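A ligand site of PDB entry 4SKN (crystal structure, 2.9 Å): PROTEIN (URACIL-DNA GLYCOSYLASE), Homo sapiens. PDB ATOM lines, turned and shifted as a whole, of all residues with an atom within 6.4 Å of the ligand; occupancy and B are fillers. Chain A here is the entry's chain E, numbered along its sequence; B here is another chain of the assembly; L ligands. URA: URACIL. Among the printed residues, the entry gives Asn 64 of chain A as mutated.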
ATOM      1  N   LEU A  61     -24.774  20.941  22.197  1.00  0.00           N
ATOM      2  CA  LEU A  61     -25.112  19.731  22.918  1.00  0.00           C
ATOM      3  C   LEU A  61     -24.593  18.480  22.210  1.00  0.00           C
ATOM      4  O   LEU A  61     -24.791  18.329  20.996  1.00  0.00           O
ATOM      5  CB  LEU A  61     -26.637  19.667  23.080  1.00  0.00           C
ATOM      6  CG  LEU A  61     -27.309  18.459  23.755  1.00  0.00           C
ATOM      7  CD1 LEU A  61     -26.878  18.308  25.202  1.00  0.00           C
ATOM      8  CD2 LEU A  61     -28.813  18.631  23.687  1.00  0.00           C
ATOM      9  N   GLY A  62     -23.885  17.635  22.965  1.00  0.00           N
ATOM     10  CA  GLY A  62     -23.364  16.367  22.449  1.00  0.00           C
ATOM     11  C   GLY A  62     -24.070  15.223  23.165  1.00  0.00           C
ATOM     12  O   GLY A  62     -25.055  15.472  23.889  1.00  0.00           O
ATOM     13  N   GLN A  63     -23.649  13.974  22.953  1.00  0.00           N
ATOM     14  CA  GLN A  63     -24.301  12.855  23.645  1.00  0.00           C
ATOM     15  C   GLN A  63     -23.704  12.465  24.989  1.00  0.00           C
ATOM     16  O   GLN A  63     -24.231  12.882  26.018  1.00  0.00           O
ATOM     17  CB  GLN A  63     -24.477  11.635  22.757  1.00  0.00           C
ATOM     18  CG  GLN A  63     -23.242  11.142  22.047  1.00  0.00           C
ATOM     19  CD  GLN A  63     -23.563   9.911  21.252  1.00  0.00           C
ATOM     20  OE1 GLN A  63     -23.140   8.807  21.589  1.00  0.00           O
ATOM     21  NE2 GLN A  63     -24.353  10.075  20.193  1.00  0.00           N
ATOM     22  N   ASN A  64     -22.632  11.673  25.008  1.00  0.00           N
ATOM     23  CA  ASN A  64     -22.011  11.295  26.284  1.00  0.00           C
ATOM     24  C   ASN A  64     -20.543  11.766  26.341  1.00  0.00           C
ATOM     25  O   ASN A  64     -19.963  12.115  25.305  1.00  0.00           O
ATOM     26  CB  ASN A  64     -22.217   9.783  26.604  1.00  0.00           C
ATOM     27  CG  ASN A  64     -21.206   8.830  25.914  1.00  0.00           C
ATOM     28  OD1 ASN A  64     -21.137   7.648  26.279  1.00  0.00           O
ATOM     29  ND2 ASN A  64     -20.470   9.320  24.923  1.00  0.00           N
ATOM     30  N   PRO A  65     -19.973  11.876  27.556  1.00  0.00           N
ATOM     31  CA  PRO A  65     -18.583  12.310  27.705  1.00  0.00           C
ATOM     32  C   PRO A  65     -17.568  11.287  27.170  1.00  0.00           C
ATOM     33  O   PRO A  65     -17.906  10.123  26.917  1.00  0.00           O
ATOM     34  CB  PRO A  65     -18.439  12.453  29.234  1.00  0.00           C
ATOM     35  CG  PRO A  65     -19.841  12.565  29.730  1.00  0.00           C
ATOM     36  CD  PRO A  65     -20.566  11.601  28.878  1.00  0.00           C
ATOM     37  N   TYR A  66     -16.312  11.721  27.039  1.00  0.00           N
ATOM     38  CA  TYR A  66     -15.248  10.847  26.568  1.00  0.00           C
ATOM     39  C   TYR A  66     -15.011   9.776  27.638  1.00  0.00           C
ATOM     40  O   TYR A  66     -14.598  10.078  28.776  1.00  0.00           O
ATOM     41  CB  TYR A  66     -13.948  11.626  26.367  1.00  0.00           C
ATOM     42  CG  TYR A  66     -13.945  12.676  25.284  1.00  0.00           C
ATOM     43  CD1 TYR A  66     -14.027  12.328  23.931  1.00  0.00           C
ATOM     44  CD2 TYR A  66     -13.768  14.020  25.600  1.00  0.00           C
ATOM     45  CE1 TYR A  66     -13.930  13.294  22.934  1.00  0.00           C
ATOM     46  CE2 TYR A  66     -13.664  14.982  24.615  1.00  0.00           C
ATOM     47  CZ  TYR A  66     -13.741  14.625  23.281  1.00  0.00           C
ATOM     48  OH  TYR A  66     -13.595  15.585  22.314  1.00  0.00           O
ATOM     49  N   ALA A  72     -12.759  13.516  29.715  1.00  0.00           N
ATOM     50  CA  ALA A  72     -13.999  14.109  30.187  1.00  0.00           C
ATOM     51  C   ALA A  72     -13.808  15.009  31.398  1.00  0.00           C
ATOM     52  O   ALA A  72     -13.390  14.545  32.454  1.00  0.00           O
ATOM     53  CB  ALA A  72     -14.990  13.004  30.500  1.00  0.00           C
ATOM     54  N   LEU A  75     -17.151  19.903  30.179  1.00  0.00           N
ATOM     55  CA  LEU A  75     -17.541  20.701  29.026  1.00  0.00           C
ATOM     56  C   LEU A  75     -17.408  19.771  27.820  1.00  0.00           C
ATOM     57  O   LEU A  75     -16.371  19.119  27.634  1.00  0.00           O
ATOM     58  CB  LEU A  75     -16.653  21.944  28.881  1.00  0.00           C
ATOM     59  CG  LEU A  75     -16.459  22.815  30.134  1.00  0.00           C
ATOM     60  CD1 LEU A  75     -15.890  24.164  29.768  1.00  0.00           C
ATOM     61  CD2 LEU A  75     -17.758  23.014  30.863  1.00  0.00           C
ATOM     62  N   CYS A  76     -18.469  19.699  27.038  1.00  0.00           N
ATOM     63  CA  CYS A  76     -18.511  18.803  25.893  1.00  0.00           C
ATOM     64  C   CYS A  76     -17.404  18.987  24.861  1.00  0.00           C
ATOM     65  O   CYS A  76     -17.146  20.109  24.419  1.00  0.00           O
ATOM     66  CB  CYS A  76     -19.887  18.885  25.210  1.00  0.00           C
ATOM     67  SG  CYS A  76     -20.325  20.513  24.563  1.00  0.00           S
ATOM     68  N   PHE A  77     -16.776  17.874  24.477  1.00  0.00           N
ATOM     69  CA  PHE A  77     -15.699  17.804  23.479  1.00  0.00           C
ATOM     70  C   PHE A  77     -14.374  18.399  23.920  1.00  0.00           C
ATOM     71  O   PHE A  77     -13.419  18.385  23.149  1.00  0.00           O
ATOM     72  CB  PHE A  77     -16.107  18.470  22.158  1.00  0.00           C
ATOM     73  CG  PHE A  77     -17.450  18.047  21.641  1.00  0.00           C
ATOM     74  CD1 PHE A  77     -17.589  16.890  20.886  1.00  0.00           C
ATOM     75  CD2 PHE A  77     -18.588  18.793  21.927  1.00  0.00           C
ATOM     76  CE1 PHE A  77     -18.851  16.488  20.428  1.00  0.00           C
ATOM     77  CE2 PHE A  77     -19.847  18.408  21.471  1.00  0.00           C
ATOM     78  CZ  PHE A  77     -19.978  17.256  20.722  1.00  0.00           C
ATOM     79  N   SER A  78     -14.305  18.846  25.172  1.00  0.00           N
ATOM     80  CA  SER A  78     -13.116  19.493  25.724  1.00  0.00           C
ATOM     81  C   SER A  78     -12.236  18.603  26.574  1.00  0.00           C
ATOM     82  O   SER A  78     -12.737  17.750  27.315  1.00  0.00           O
ATOM     83  CB  SER A  78     -13.574  20.673  26.581  1.00  0.00           C
ATOM     84  OG  SER A  78     -12.480  21.494  26.911  1.00  0.00           O
ATOM     85  N   SER A  88     -12.799  14.016  17.829  1.00  0.00           N
ATOM     86  CA  SER A  88     -13.973  14.889  17.761  1.00  0.00           C
ATOM     87  C   SER A  88     -13.604  16.364  17.828  1.00  0.00           C
ATOM     88  O   SER A  88     -14.196  17.170  17.107  1.00  0.00           O
ATOM     89  CB  SER A  88     -14.953  14.549  18.886  1.00  0.00           C
ATOM     90  OG  SER A  88     -15.475  13.247  18.711  1.00  0.00           O
ATOM     91  N   LEU A 122     -23.082  21.588  26.849  1.00  0.00           N
ATOM     92  CA  LEU A 122     -23.826  20.477  27.453  1.00  0.00           C
ATOM     93  C   LEU A 122     -23.624  19.162  26.723  1.00  0.00           C
ATOM     94  O   LEU A 122     -23.015  19.111  25.649  1.00  0.00           O
ATOM     95  CB  LEU A 122     -25.319  20.827  27.485  1.00  0.00           C
ATOM     96  CG  LEU A 122     -26.256  20.026  28.378  1.00  0.00           C
ATOM     97  CD1 LEU A 122     -25.895  20.230  29.843  1.00  0.00           C
ATOM     98  CD2 LEU A 122     -27.684  20.466  28.131  1.00  0.00           C
ATOM     99  N   ASN A 123     -24.153  18.105  27.312  1.00  0.00           N
ATOM    100  CA  ASN A 123     -24.087  16.748  26.770  1.00  0.00           C
ATOM    101  C   ASN A 123     -25.372  16.134  27.279  1.00  0.00           C
ATOM    102  O   ASN A 123     -25.798  16.467  28.382  1.00  0.00           O
ATOM    103  CB  ASN A 123     -22.906  16.004  27.372  1.00  0.00           C
ATOM    104  CG  ASN A 123     -21.853  15.663  26.352  1.00  0.00           C
ATOM    105  OD1 ASN A 123     -22.010  15.898  25.160  1.00  0.00           O
ATOM    106  ND2 ASN A 123     -20.744  15.106  26.829  1.00  0.00           N
ATOM    107  N   ALA A 124     -25.987  15.244  26.499  1.00  0.00           N
ATOM    108  CA  ALA A 124     -27.227  14.598  26.902  1.00  0.00           C
ATOM    109  C   ALA A 124     -27.067  13.798  28.173  1.00  0.00           C
ATOM    110  O   ALA A 124     -27.829  13.965  29.127  1.00  0.00           O
ATOM    111  CB  ALA A 124     -27.725  13.712  25.812  1.00  0.00           C
ATOM    112  N   TRP A 164     -25.684  18.353  17.852  1.00  0.00           N
ATOM    113  CA  TRP A 164     -24.793  17.502  17.103  1.00  0.00           C
ATOM    114  C   TRP A 164     -24.968  16.013  17.394  1.00  0.00           C
ATOM    115  O   TRP A 164     -24.581  15.529  18.455  1.00  0.00           O
ATOM    116  CB  TRP A 164     -23.353  17.944  17.350  1.00  0.00           C
ATOM    117  CG  TRP A 164     -23.068  19.350  16.873  1.00  0.00           C
ATOM    118  CD1 TRP A 164     -23.890  20.145  16.136  1.00  0.00           C
ATOM    119  CD2 TRP A 164     -21.879  20.123  17.117  1.00  0.00           C
ATOM    120  NE1 TRP A 164     -23.299  21.356  15.892  1.00  0.00           N
ATOM    121  CE2 TRP A 164     -22.052  21.365  16.477  1.00  0.00           C
ATOM    122  CE3 TRP A 164     -20.684  19.879  17.789  1.00  0.00           C
ATOM    123  CZ2 TRP A 164     -21.073  22.358  16.498  1.00  0.00           C
ATOM    124  CZ3 TRP A 164     -19.711  20.879  17.815  1.00  0.00           C
ATOM    125  CH2 TRP A 164     -19.916  22.101  17.179  1.00  0.00           C
ATOM    126  N   HIS A 187     -22.886  14.133  14.412  1.00  0.00           N
ATOM    127  CA  HIS A 187     -21.944  14.235  15.521  1.00  0.00           C
ATOM    128  C   HIS A 187     -20.523  14.245  14.935  1.00  0.00           C
ATOM    129  O   HIS A 187     -20.174  13.400  14.114  1.00  0.00           O
ATOM    130  CB  HIS A 187     -22.135  13.059  16.473  1.00  0.00           C
ATOM    131  CG  HIS A 187     -21.181  13.052  17.633  1.00  0.00           C
ATOM    132  ND1 HIS A 187     -19.879  12.616  17.522  1.00  0.00           N
ATOM    133  CD2 HIS A 187     -21.348  13.403  18.926  1.00  0.00           C
ATOM    134  CE1 HIS A 187     -19.282  12.705  18.693  1.00  0.00           C
ATOM    135  NE2 HIS A 187     -20.151  13.169  19.567  1.00  0.00           N
ATOM    136  C1  ORP B   5     -18.958  10.167  22.559  1.00  0.00           C
ATOM    137  O1  ORP B   5     -19.510   7.888  22.858  1.00  0.00           O
ATOM    138  C2  ORP B   5     -19.140  10.452  21.081  1.00  0.00           C
ATOM    139  C3  ORP B   5     -18.162   9.519  20.405  1.00  0.00           C
ATOM    140  O3  ORP B   5     -18.746   8.231  20.193  1.00  0.00           O
ATOM    141  C4  ORP B   5     -17.027   9.417  21.421  1.00  0.00           C
ATOM    142  O4  ORP B   5     -17.640   9.649  22.718  1.00  0.00           O
ATOM    143  C5  ORP B   5     -15.873  10.377  21.216  1.00  0.00           C
ATOM    144  O5  ORP B   5     -15.067   9.957  20.099  1.00  0.00           O
ATOM    145  P   ORP B   5     -13.520  10.324  20.017  1.00  0.00           P
ATOM    146  O1P ORP B   5     -13.392  11.621  19.306  1.00  0.00           O
ATOM    147  O2P ORP B   5     -12.882  10.166  21.349  1.00  0.00           O
ATOM    148  P    DG B   6     -19.017   7.707  18.690  1.00  0.00           P
ATOM    149  OP1  DG B   6     -20.000   6.593  18.816  1.00  0.00           O
ATOM    150  OP2  DG B   6     -17.699   7.443  18.026  1.00  0.00           O
ATOM    151  O5'  DG B   6     -19.726   8.945  17.956  1.00  0.00           O
ATOM    152  C5'  DG B   6     -21.161   9.042  17.842  1.00  0.00           C
ATOM    153  C4'  DG B   6     -21.553   9.368  16.413  1.00  0.00           C
ATOM    154  O4'  DG B   6     -21.016   8.336  15.555  1.00  0.00           O
ATOM    155  C3'  DG B   6     -23.054   9.396  16.115  1.00  0.00           C
ATOM    156  O3'  DG B   6     -23.328  10.356  15.074  1.00  0.00           O
ATOM    157  C2'  DG B   6     -23.346   7.984  15.650  1.00  0.00           C
ATOM    158  C1'  DG B   6     -22.053   7.600  14.941  1.00  0.00           C
ATOM    159  N9   DG B   6     -21.714   6.193  15.051  1.00  0.00           N
ATOM    160  C8   DG B   6     -21.291   5.518  16.173  1.00  0.00           C
ATOM    161  N7   DG B   6     -21.006   4.266  15.953  1.00  0.00           N
ATOM    162  C5   DG B   6     -21.276   4.098  14.603  1.00  0.00           C
ATOM    163  C6   DG B   6     -21.163   2.955  13.787  1.00  0.00           C
ATOM    164  O6   DG B   6     -20.764   1.822  14.107  1.00  0.00           O
ATOM    165  N1   DG B   6     -21.544   3.215  12.477  1.00  0.00           N
ATOM    166  C2   DG B   6     -21.986   4.435  12.011  1.00  0.00           C
ATOM    167  N2   DG B   6     -22.293   4.507  10.702  1.00  0.00           N
ATOM    168  N3   DG B   6     -22.101   5.510  12.764  1.00  0.00           N
ATOM    169  C4   DG B   6     -21.738   5.275  14.040  1.00  0.00           C
HETATM  170  N1  URA L   1     -18.956  13.147  22.438  1.00  0.00           N
HETATM  171  C2  URA L   1     -19.906  13.874  23.119  1.00  0.00           C
HETATM  172  O2  URA L   1     -21.089  13.835  22.845  1.00  0.00           O
HETATM  173  N3  URA L   1     -19.418  14.646  24.155  1.00  0.00           N
HETATM  174  C4  URA L   1     -18.103  14.721  24.578  1.00  0.00           C
HETATM  175  O4  URA L   1     -17.826  15.358  25.610  1.00  0.00           O
HETATM  176  C5  URA L   1     -17.182  13.927  23.817  1.00  0.00           C
HETATM  177  C6  URA L   1     -17.637  13.196  22.795  1.00  0.00           C
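C of Gly 62 touches O2 of the ligand, at 3.3 Å. Pro 65 touches the ligand (CA to O4, 3.8 Å). Tyr 66 touches the ligand (CE1 to C5, 3.4 Å). CA of Cys 76 touches O4 of the ligand (3.5 Å). ORP 5 of chain B touches the ligand (C1 to N1, 3.0 Å).
NE2 of His 187 lies within hydrogen-bond range of N1 of the ligand, 3.1 Å away. The side-chain amide nitrogen (ND2) of Asn 123 sits close to a nitrogen (N3) of the ligand, 3.0 Å away. The backbone NH (N) of Gln 63 is in hydrogen-bond range of an oxygen (O2) of the ligand, 2.6 Å away. O of Asn 64 sits close to N3 of the ligand, at 2.8 Å. The backbone NH of Asn 64 is in hydrogen-bond range of an oxygen (O2) of the ligand, 3.4 Å away. An oxygen (O4) of the ligand is in hydrogen-bond range of the backbone NH (N) of Phe 77 (3.0 Å).
The backbone NH of Gly 62 lies within hydrogen-bond range of the backbone carbonyl oxygen of Leu 122 (3.2 Å). O1 of ORP 5 of chain B sits at hydrogen-bond distance from ND2 of Asn 64, at 2.7 Å. OH of Tyr 66 lies within hydrogen-bond range of O of Phe 77. The side-chain sulfur (SG) of Cys 76 sits close to the backbone carbonyl oxygen (O) of Leu 122 (3.2 Å). O of Gly 62 sits close to OD1 of Asn 123 (3.3 Å). O1P of ORP 5 of chain B lies within hydrogen-bond range of the side-chain hydroxyl (OG) of Ser 88, 2.7 Å away. The backbone NH (N) of Gln 63 is in hydrogen-bond range of the side-chain amide oxygen (OD1) of Asn 123 (3.4 Å). The backbone carbonyl oxygen (O) of Asn 64 sits close to the side-chain amide nitrogen (ND2) of Asn 123, at 3.4 Å.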
